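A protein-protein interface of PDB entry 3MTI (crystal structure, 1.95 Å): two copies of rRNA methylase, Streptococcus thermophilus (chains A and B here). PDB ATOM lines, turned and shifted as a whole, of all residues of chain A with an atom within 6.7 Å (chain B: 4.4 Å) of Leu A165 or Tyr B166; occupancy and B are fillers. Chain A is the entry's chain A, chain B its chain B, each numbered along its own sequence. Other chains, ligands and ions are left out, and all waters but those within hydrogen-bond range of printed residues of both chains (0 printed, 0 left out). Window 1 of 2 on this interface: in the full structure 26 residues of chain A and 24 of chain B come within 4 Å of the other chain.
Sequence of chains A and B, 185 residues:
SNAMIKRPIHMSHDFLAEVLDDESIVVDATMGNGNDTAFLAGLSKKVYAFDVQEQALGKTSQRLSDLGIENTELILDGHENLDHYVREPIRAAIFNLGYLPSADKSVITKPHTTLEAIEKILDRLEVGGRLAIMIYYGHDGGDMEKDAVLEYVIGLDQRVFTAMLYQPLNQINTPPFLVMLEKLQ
The backbone carbonyl oxygen (O) of Gln A167 sits at hydrogen-bond distance from the backbone NH (N) of Leu B165 (2.7 Å).
The backbone NH of Leu A165 sits at hydrogen-bond distance from the backbone carbonyl oxygen of Gln B167 (2.7 Å).
O of Ala A163 sits at hydrogen-bond distance from N of Leu B169, at 2.8 Å.
The backbone carbonyl oxygen (O) of Leu A165 lies close to the backbone carbonyl oxygen (O) of Leu B165 (3.4 Å).
N of Leu B178 is in hydrogen-bond range of O of Tyr B166, at 2.9 Å.
N of Leu A178 is in hydrogen-bond range of O of Tyr A166 (2.9 Å).
The backbone carbonyl oxygen of Lys B6 sits at hydrogen-bond distance from the side-chain hydroxyl of Tyr B166 (2.6 Å).
The backbone NH of Met B164 sits at hydrogen-bond distance from the backbone carbonyl oxygen of Met B180 (2.9 Å).
O of Met A164 sits at hydrogen-bond distance from N of Met A180 (2.8 Å).
Among the printed residues, merely in contact across the chains: Leu A165 with Tyr B166 (3.1 Å), Tyr A166 with Leu B165 (3.2 Å), Gln A167 with Met B164 (3.3 Å), Met A164 with Gln B167 (3.3 Å), Met A164 with Tyr B166 (3.4 Å), Tyr A166 with Met B164 (3.4 Å), Leu A169 with Leu B165 (3.9 Å), Leu A165 with Leu B169 (3.9 Å), Leu A169 with Met B164 (3.9 Å), Val A179 with Leu B169 (3.9 Å), Met A180 with Tyr B166 (3.9 Å), Tyr A166 with Met B180 (3.95 Å) and Tyr A166 with Tyr B166 (3.97 Å).
Leu A165 touches just these residues of chain B: Leu B165 (3.4 Å), Tyr B166 (3.1 Å), Gln B167 (2.7 Å) and Leu B169 (3.9 Å).
Printed residues of chain B within 4 Å of Gln A167: Met B164 and Leu B165.
Of the printed residues of chain B, Leu A169 touches Met B164 (3.9 Å) and Leu B165 (3.9 Å).
Printed residues of chain B within 4 Å of Val A179: Leu B169.
Printed residues of chain B within 4 Å of Met A180: Tyr B166 (3.9 Å).
Of chain A, only Met A164, Leu A165, Tyr A166 and Met A180 come within 4 Å of Tyr B166.
Of the printed residues of chain A, Met B180 touches Tyr A166 (3.95 Å).
The nearest printed residue of chain B that does not touch Leu A165 is Leu B178 (6.8 Å).
The nearest printed residue of chain B that does not touch Tyr A166 is Gln B167 (5.1 Å).
Of the 12 printed residues of chain B, 6 touch a printed residue of chain A.
Hydrophobic or aromatic side chains of chain B within 4 Å of the printed part of chain A: Met B164, Leu B165, Tyr B166, Leu B169 and Met B180.
Printed residues of chain A that touch a printed residue of chain B: Ala A163, Met A164, Leu A165, Tyr A166, Gln A167, Leu A169, Val A179 and Met A180.
Hydrophobic or aromatic side chains of chain A within 4 Å of the printed part of chain B: Met A164, Leu A165, Tyr A166, Leu A169, Val A179 and Met A180.
Among the printed residues, no Asp or Glu carboxylate lies within 4 Å of a Lys or Arg side-chain nitrogen of the other chain.
Met A164 touches Gln B167, and with the chains exchanged Gln A167 touches Met B164.
Leu A165 touches Tyr B166, and with the chains exchanged Tyr A166 touches Leu B165.
Leu A165 touches Gln B167, and with the chains exchanged Gln A167 touches Leu B165.
Tyr A166 touches its own counterpart, Tyr B166.
Of the 17 pairs that touch across the chains among the printed residues, 14 have their exchanged pair printed and touching as well.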
ATOM      1  N   MET A  11     -11.417 -26.185  -0.808  1.00  0.00           N
ATOM      2  CA  MET A  11     -10.753 -25.728  -2.014  1.00  0.00           C
ATOM      3  C   MET A  11      -9.336 -25.226  -1.734  1.00  0.00           C
ATOM      4  O   MET A  11      -8.429 -25.471  -2.517  1.00  0.00           O
ATOM      5  CB  MET A  11     -11.570 -24.616  -2.685  1.00  0.00           C
ATOM      6  CG  MET A  11     -10.961 -24.106  -3.992  1.00  0.00           C
ATOM      7  SD  MET A  11     -11.049 -25.361  -5.500  1.00  0.00           S
ATOM      8  CE  MET A  11     -12.882 -25.013  -6.104  1.00  0.00           C
ATOM      9  N   PHE A  15      -6.203 -26.979  -3.415  1.00  0.00           N
ATOM     10  CA  PHE A  15      -5.377 -26.071  -4.220  1.00  0.00           C
ATOM     11  C   PHE A  15      -3.904 -26.188  -3.839  1.00  0.00           C
ATOM     12  O   PHE A  15      -3.030 -26.311  -4.687  1.00  0.00           O
ATOM     13  CB  PHE A  15      -5.858 -24.640  -3.982  1.00  0.00           C
ATOM     14  CG  PHE A  15      -5.123 -23.596  -4.749  1.00  0.00           C
ATOM     15  CD1 PHE A  15      -5.240 -23.516  -6.141  1.00  0.00           C
ATOM     16  CD2 PHE A  15      -4.401 -22.629  -4.080  1.00  0.00           C
ATOM     17  CE1 PHE A  15      -4.599 -22.525  -6.841  1.00  0.00           C
ATOM     18  CE2 PHE A  15      -3.738 -21.617  -4.779  1.00  0.00           C
ATOM     19  CZ  PHE A  15      -3.847 -21.559  -6.159  1.00  0.00           C
ATOM     20  N   LEU A 150      -7.093  -7.185  -0.796  1.00  0.00           N
ATOM     21  CA  LEU A 150      -7.764  -7.356  -2.076  1.00  0.00           C
ATOM     22  C   LEU A 150      -7.273  -6.455  -3.203  1.00  0.00           C
ATOM     23  O   LEU A 150      -7.136  -6.930  -4.332  1.00  0.00           O
ATOM     24  CB  LEU A 150      -9.277  -7.251  -1.934  1.00  0.00           C
ATOM     25  CG  LEU A 150      -9.962  -8.406  -2.660  1.00  0.00           C
ATOM     26  CD1 LEU A 150      -9.864  -9.696  -1.815  1.00  0.00           C
ATOM     27  CD2 LEU A 150     -11.419  -8.044  -2.980  1.00  0.00           C
ATOM     28  N   ALA A 163      -4.527 -14.745 -10.228  1.00  0.00           N
ATOM     29  CA  ALA A 163      -5.310 -14.516  -9.031  1.00  0.00           C
ATOM     30  C   ALA A 163      -6.782 -14.861  -9.257  1.00  0.00           C
ATOM     31  O   ALA A 163      -7.472 -14.242 -10.081  1.00  0.00           O
ATOM     32  CB  ALA A 163      -5.163 -13.070  -8.573  1.00  0.00           C
ATOM     33  N   MET A 164      -7.265 -15.839  -8.499  1.00  0.00           N
ATOM     34  CA  MET A 164      -8.649 -16.284  -8.610  1.00  0.00           C
ATOM     35  C   MET A 164      -9.419 -16.093  -7.311  1.00  0.00           C
ATOM     36  O   MET A 164      -8.897 -16.333  -6.190  1.00  0.00           O
ATOM     37  CB  MET A 164      -8.716 -17.747  -9.065  1.00  0.00           C
ATOM     38  CG  MET A 164      -7.968 -18.052 -10.362  1.00  0.00           C
ATOM     39  SD  MET A 164      -8.846 -17.288 -11.982  1.00  0.00           S
ATOM     40  CE  MET A 164     -10.641 -17.736 -11.516  1.00  0.00           C
ATOM     41  N   LEU A 165     -10.664 -15.659  -7.475  1.00  0.00           N
ATOM     42  CA  LEU A 165     -11.629 -15.518  -6.395  1.00  0.00           C
ATOM     43  C   LEU A 165     -12.556 -16.720  -6.377  1.00  0.00           C
ATOM     44  O   LEU A 165     -13.090 -17.114  -7.410  1.00  0.00           O
ATOM     45  CB  LEU A 165     -12.459 -14.219  -6.531  1.00  0.00           C
ATOM     46  CG  LEU A 165     -13.590 -13.973  -5.499  1.00  0.00           C
ATOM     47  CD1 LEU A 165     -13.064 -13.881  -4.043  1.00  0.00           C
ATOM     48  CD2 LEU A 165     -14.453 -12.723  -5.806  1.00  0.00           C
ATOM     49  N   TYR A 166     -12.726 -17.310  -5.196  1.00  0.00           N
ATOM     50  CA  TYR A 166     -13.663 -18.396  -5.009  1.00  0.00           C
ATOM     51  C   TYR A 166     -14.516 -18.083  -3.765  1.00  0.00           C
ATOM     52  O   TYR A 166     -14.034 -18.095  -2.611  1.00  0.00           O
ATOM     53  CB  TYR A 166     -12.922 -19.740  -4.949  1.00  0.00           C
ATOM     54  CG  TYR A 166     -13.814 -20.958  -4.832  1.00  0.00           C
ATOM     55  CD1 TYR A 166     -14.644 -21.349  -5.875  1.00  0.00           C
ATOM     56  CD2 TYR A 166     -13.810 -21.730  -3.673  1.00  0.00           C
ATOM     57  CE1 TYR A 166     -15.470 -22.474  -5.763  1.00  0.00           C
ATOM     58  CE2 TYR A 166     -14.612 -22.850  -3.547  1.00  0.00           C
ATOM     59  CZ  TYR A 166     -15.440 -23.226  -4.584  1.00  0.00           C
ATOM     60  OH  TYR A 166     -16.235 -24.335  -4.447  1.00  0.00           O
ATOM     61  N   GLN A 167     -15.780 -17.759  -4.016  1.00  0.00           N
ATOM     62  CA  GLN A 167     -16.623 -17.089  -3.016  1.00  0.00           C
ATOM     63  C   GLN A 167     -18.048 -17.638  -3.022  1.00  0.00           C
ATOM     64  O   GLN A 167     -18.616 -17.830  -4.085  1.00  0.00           O
ATOM     65  CB  GLN A 167     -16.635 -15.577  -3.307  1.00  0.00           C
ATOM     66  CG  GLN A 167     -17.483 -14.723  -2.360  1.00  0.00           C
ATOM     67  CD  GLN A 167     -17.313 -13.244  -2.624  1.00  0.00           C
ATOM     68  OE1 GLN A 167     -17.672 -12.749  -3.687  1.00  0.00           O
ATOM     69  NE2 GLN A 167     -16.732 -12.526  -1.651  1.00  0.00           N
ATOM     70  N   LEU A 169     -22.040 -17.500  -2.928  1.00  0.00           N
ATOM     71  CA  LEU A 169     -22.964 -16.460  -3.411  1.00  0.00           C
ATOM     72  C   LEU A 169     -24.227 -16.330  -2.580  1.00  0.00           C
ATOM     73  O   LEU A 169     -24.626 -15.223  -2.226  1.00  0.00           O
ATOM     74  CB  LEU A 169     -23.332 -16.711  -4.871  1.00  0.00           C
ATOM     75  CG  LEU A 169     -22.258 -16.359  -5.895  1.00  0.00           C
ATOM     76  CD1 LEU A 169     -22.659 -16.883  -7.265  1.00  0.00           C
ATOM     77  CD2 LEU A 169     -21.985 -14.819  -5.911  1.00  0.00           C
ATOM     78  N   PHE A 177     -14.340 -16.377   2.187  1.00  0.00           N
ATOM     79  CA  PHE A 177     -13.995 -16.671   0.798  1.00  0.00           C
ATOM     80  C   PHE A 177     -12.498 -16.845   0.606  1.00  0.00           C
ATOM     81  O   PHE A 177     -11.688 -16.494   1.474  1.00  0.00           O
ATOM     82  CB  PHE A 177     -14.527 -15.583  -0.154  1.00  0.00           C
ATOM     83  CG  PHE A 177     -13.894 -14.238   0.037  1.00  0.00           C
ATOM     84  CD1 PHE A 177     -12.759 -13.885  -0.677  1.00  0.00           C
ATOM     85  CD2 PHE A 177     -14.454 -13.314   0.915  1.00  0.00           C
ATOM     86  CE1 PHE A 177     -12.179 -12.632  -0.513  1.00  0.00           C
ATOM     87  CE2 PHE A 177     -13.896 -12.060   1.090  1.00  0.00           C
ATOM     88  CZ  PHE A 177     -12.753 -11.707   0.379  1.00  0.00           C
ATOM     89  N   LEU A 178     -12.140 -17.364  -0.557  1.00  0.00           N
ATOM     90  CA  LEU A 178     -10.761 -17.717  -0.858  1.00  0.00           C
ATOM     91  C   LEU A 178     -10.192 -16.944  -2.034  1.00  0.00           C
ATOM     92  O   LEU A 178     -10.865 -16.743  -3.059  1.00  0.00           O
ATOM     93  CB  LEU A 178     -10.649 -19.227  -1.111  1.00  0.00           C
ATOM     94  CG  LEU A 178      -9.381 -19.867  -1.705  1.00  0.00           C
ATOM     95  CD1 LEU A 178      -8.167 -19.748  -0.771  1.00  0.00           C
ATOM     96  CD2 LEU A 178      -9.669 -21.354  -2.042  1.00  0.00           C
ATOM     97  N   VAL A 179      -8.952 -16.500  -1.850  1.00  0.00           N
ATOM     98  CA  VAL A 179      -8.099 -15.965  -2.909  1.00  0.00           C
ATOM     99  C   VAL A 179      -6.989 -16.976  -3.181  1.00  0.00           C
ATOM    100  O   VAL A 179      -6.222 -17.360  -2.277  1.00  0.00           O
ATOM    101  CB  VAL A 179      -7.465 -14.607  -2.501  1.00  0.00           C
ATOM    102  CG1 VAL A 179      -6.693 -13.993  -3.649  1.00  0.00           C
ATOM    103  CG2 VAL A 179      -8.520 -13.650  -1.964  1.00  0.00           C
ATOM    104  N   MET A 180      -6.930 -17.407  -4.431  1.00  0.00           N
ATOM    105  CA  MET A 180      -5.956 -18.368  -4.925  1.00  0.00           C
ATOM    106  C   MET A 180      -4.931 -17.644  -5.769  1.00  0.00           C
ATOM    107  O   MET A 180      -5.295 -16.931  -6.727  1.00  0.00           O
ATOM    108  CB  MET A 180      -6.647 -19.430  -5.791  1.00  0.00           C
ATOM    109  CG  MET A 180      -7.399 -20.497  -5.003  1.00  0.00           C
ATOM    110  SD  MET A 180      -8.969 -21.121  -5.997  1.00  0.00           S
ATOM    111  CE  MET A 180      -8.098 -22.068  -7.449  1.00  0.00           C
ATOM    112  N   LYS B   6      -6.892 -23.275 -12.846  1.00  0.00           N
ATOM    113  CA  LYS B   6      -7.866 -23.442 -13.938  1.00  0.00           C
ATOM    114  C   LYS B   6      -8.516 -22.132 -14.391  1.00  0.00           C
ATOM    115  O   LYS B   6      -9.059 -21.386 -13.590  1.00  0.00           O
ATOM    116  CB  LYS B   6      -8.960 -24.467 -13.573  1.00  0.00           C
ATOM    117  CG  LYS B   6      -8.461 -25.874 -13.280  1.00  0.00           C
ATOM    118  CD  LYS B   6      -9.441 -26.638 -12.401  1.00  0.00           C
ATOM    119  CE  LYS B   6      -8.786 -27.889 -11.802  1.00  0.00           C
ATOM    120  NZ  LYS B   6      -8.972 -27.892 -10.312  1.00  0.00           N
ATOM    121  N   ARG B   7      -8.471 -21.854 -15.687  1.00  0.00           N
ATOM    122  CA  ARG B   7      -9.320 -20.788 -16.229  1.00  0.00           C
ATOM    123  C   ARG B   7     -10.764 -21.149 -15.894  1.00  0.00           C
ATOM    124  O   ARG B   7     -11.060 -22.328 -15.745  1.00  0.00           O
ATOM    125  CB  ARG B   7      -9.117 -20.643 -17.748  1.00  0.00           C
ATOM    126  CG  ARG B   7      -7.857 -19.885 -18.106  1.00  0.00           C
ATOM    127  CD  ARG B   7      -7.752 -19.501 -19.601  1.00  0.00           C
ATOM    128  NE  ARG B   7      -8.218 -20.528 -20.543  1.00  0.00           N
ATOM    129  CZ  ARG B   7      -7.553 -21.639 -20.843  1.00  0.00           C
ATOM    130  NH1 ARG B   7      -6.380 -21.918 -20.266  1.00  0.00           N
ATOM    131  NH2 ARG B   7      -8.064 -22.484 -21.723  1.00  0.00           N
ATOM    132  N   PRO B   8     -11.668 -20.143 -15.775  1.00  0.00           N
ATOM    133  CA  PRO B   8     -13.077 -20.419 -15.463  1.00  0.00           C
ATOM    134  C   PRO B   8     -13.715 -21.496 -16.360  1.00  0.00           C
ATOM    135  O   PRO B   8     -14.598 -22.223 -15.914  1.00  0.00           O
ATOM    136  CB  PRO B   8     -13.755 -19.056 -15.693  1.00  0.00           C
ATOM    137  CG  PRO B   8     -12.683 -18.063 -15.425  1.00  0.00           C
ATOM    138  CD  PRO B   8     -11.443 -18.690 -15.988  1.00  0.00           C
ATOM    139  N   MET B  11     -12.542 -24.914 -15.239  1.00  0.00           N
ATOM    140  CA  MET B  11     -13.210 -25.222 -13.973  1.00  0.00           C
ATOM    141  C   MET B  11     -14.661 -25.632 -14.215  1.00  0.00           C
ATOM    142  O   MET B  11     -15.139 -26.547 -13.579  1.00  0.00           O
ATOM    143  CB  MET B  11     -13.079 -24.065 -12.974  1.00  0.00           C
ATOM    144  CG  MET B  11     -13.875 -24.218 -11.698  1.00  0.00           C
ATOM    145  SD  MET B  11     -12.951 -25.483 -10.483  1.00  0.00           S
ATOM    146  CE  MET B  11     -11.502 -24.346  -9.863  1.00  0.00           C
ATOM    147  N   MET B 164     -21.540 -20.918  -5.999  1.00  0.00           N
ATOM    148  CA  MET B 164     -20.196 -20.382  -5.843  1.00  0.00           C
ATOM    149  C   MET B 164     -19.797 -19.511  -7.026  1.00  0.00           C
ATOM    150  O   MET B 164     -20.124 -19.809  -8.186  1.00  0.00           O
ATOM    151  CB  MET B 164     -19.162 -21.514  -5.720  1.00  0.00           C
ATOM    152  CG  MET B 164     -19.403 -22.521  -4.610  1.00  0.00           C
ATOM    153  SD  MET B 164     -19.075 -21.832  -2.794  1.00  0.00           S
ATOM    154  CE  MET B 164     -17.420 -20.885  -3.027  1.00  0.00           C
ATOM    155  N   LEU B 165     -19.062 -18.450  -6.715  1.00  0.00           N
ATOM    156  CA  LEU B 165     -18.456 -17.587  -7.715  1.00  0.00           C
ATOM    157  C   LEU B 165     -16.978 -17.931  -7.815  1.00  0.00           C
ATOM    158  O   LEU B 165     -16.279 -18.041  -6.792  1.00  0.00           O
ATOM    159  CB  LEU B 165     -18.639 -16.107  -7.361  1.00  0.00           C
ATOM    160  CG  LEU B 165     -17.949 -15.046  -8.233  1.00  0.00           C
ATOM    161  CD1 LEU B 165     -18.606 -14.927  -9.620  1.00  0.00           C
ATOM    162  CD2 LEU B 165     -17.920 -13.679  -7.545  1.00  0.00           C
ATOM    163  N   TYR B 166     -16.541 -18.148  -9.044  1.00  0.00           N
ATOM    164  CA  TYR B 166     -15.146 -18.385  -9.379  1.00  0.00           C
ATOM    165  C   TYR B 166     -14.742 -17.382 -10.452  1.00  0.00           C
ATOM    166  O   TYR B 166     -15.242 -17.434 -11.592  1.00  0.00           O
ATOM    167  CB  TYR B 166     -14.955 -19.829  -9.848  1.00  0.00           C
ATOM    168  CG  TYR B 166     -13.528 -20.221 -10.145  1.00  0.00           C
ATOM    169  CD1 TYR B 166     -12.582 -20.349  -9.119  1.00  0.00           C
ATOM    170  CD2 TYR B 166     -13.128 -20.517 -11.444  1.00  0.00           C
ATOM    171  CE1 TYR B 166     -11.273 -20.724  -9.395  1.00  0.00           C
ATOM    172  CE2 TYR B 166     -11.842 -20.900 -11.728  1.00  0.00           C
ATOM    173  CZ  TYR B 166     -10.911 -21.003 -10.706  1.00  0.00           C
ATOM    174  OH  TYR B 166      -9.628 -21.391 -11.010  1.00  0.00           O
ATOM    175  N   GLN B 167     -13.877 -16.441 -10.082  1.00  0.00           N
ATOM    176  CA  GLN B 167     -13.547 -15.343 -10.999  1.00  0.00           C
ATOM    177  C   GLN B 167     -12.121 -14.809 -10.890  1.00  0.00           C
ATOM    178  O   GLN B 167     -11.570 -14.726  -9.788  1.00  0.00           O
ATOM    179  CB  GLN B 167     -14.564 -14.207 -10.878  1.00  0.00           C
ATOM    180  CG  GLN B 167     -14.198 -13.119  -9.942  1.00  0.00           C
ATOM    181  CD  GLN B 167     -14.963 -11.846 -10.198  1.00  0.00           C
ATOM    182  OE1 GLN B 167     -15.701 -11.379  -9.346  1.00  0.00           O
ATOM    183  NE2 GLN B 167     -14.794 -11.282 -11.382  1.00  0.00           N
ATOM    184  N   LEU B 169      -9.213 -12.181 -10.614  1.00  0.00           N
ATOM    185  CA  LEU B 169      -9.172 -10.916  -9.888  1.00  0.00           C
ATOM    186  C   LEU B 169      -8.278  -9.865 -10.539  1.00  0.00           C
ATOM    187  O   LEU B 169      -8.461  -8.659 -10.336  1.00  0.00           O
ATOM    188  CB  LEU B 169      -8.693 -11.143  -8.436  1.00  0.00           C
ATOM    189  CG  LEU B 169      -9.734 -11.590  -7.391  1.00  0.00           C
ATOM    190  CD1 LEU B 169      -9.058 -12.033  -6.044  1.00  0.00           C
ATOM    191  CD2 LEU B 169     -10.794 -10.508  -7.137  1.00  0.00           C
ATOM    192  N   PHE B 177     -16.399 -14.991 -15.961  1.00  0.00           N
ATOM    193  CA  PHE B 177     -16.488 -15.575 -14.631  1.00  0.00           C
ATOM    194  C   PHE B 177     -17.500 -16.713 -14.606  1.00  0.00           C
ATOM    195  O   PHE B 177     -18.375 -16.814 -15.481  1.00  0.00           O
ATOM    196  CB  PHE B 177     -16.808 -14.514 -13.556  1.00  0.00           C
ATOM    197  CG  PHE B 177     -18.116 -13.809 -13.749  1.00  0.00           C
ATOM    198  CD1 PHE B 177     -19.243 -14.216 -13.056  1.00  0.00           C
ATOM    199  CD2 PHE B 177     -18.210 -12.706 -14.604  1.00  0.00           C
ATOM    200  CE1 PHE B 177     -20.460 -13.560 -13.218  1.00  0.00           C
ATOM    201  CE2 PHE B 177     -19.420 -12.039 -14.782  1.00  0.00           C
ATOM    202  CZ  PHE B 177     -20.546 -12.460 -14.089  1.00  0.00           C
ATOM    203  N   LEU B 178     -17.373 -17.558 -13.583  1.00  0.00           N
ATOM    204  CA  LEU B 178     -18.174 -18.765 -13.484  1.00  0.00           C
ATOM    205  C   LEU B 178     -19.075 -18.815 -12.232  1.00  0.00           C
ATOM    206  O   LEU B 178     -18.661 -18.471 -11.101  1.00  0.00           O
ATOM    207  CB  LEU B 178     -17.258 -20.007 -13.599  1.00  0.00           C
ATOM    208  CG  LEU B 178     -17.713 -21.402 -13.147  1.00  0.00           C
ATOM    209  CD1 LEU B 178     -18.906 -21.887 -13.975  1.00  0.00           C
ATOM    210  CD2 LEU B 178     -16.541 -22.424 -13.200  1.00  0.00           C
ATOM    211  N   MET B 180     -21.063 -21.683 -10.157  1.00  0.00           N
ATOM    212  CA  MET B 180     -21.188 -23.118  -9.923  1.00  0.00           C
ATOM    213  C   MET B 180     -22.383 -23.378  -9.010  1.00  0.00           C
ATOM    214  O   MET B 180     -22.422 -22.861  -7.897  1.00  0.00           O
ATOM    215  CB  MET B 180     -19.904 -23.643  -9.269  1.00  0.00           C
ATOM    216  CG  MET B 180     -18.693 -23.616 -10.214  1.00  0.00           C
ATOM    217  SD  MET B 180     -17.000 -23.371  -9.297  1.00  0.00           S
ATOM    218  CE  MET B 180     -16.811 -25.108  -8.416  1.00  0.00           C
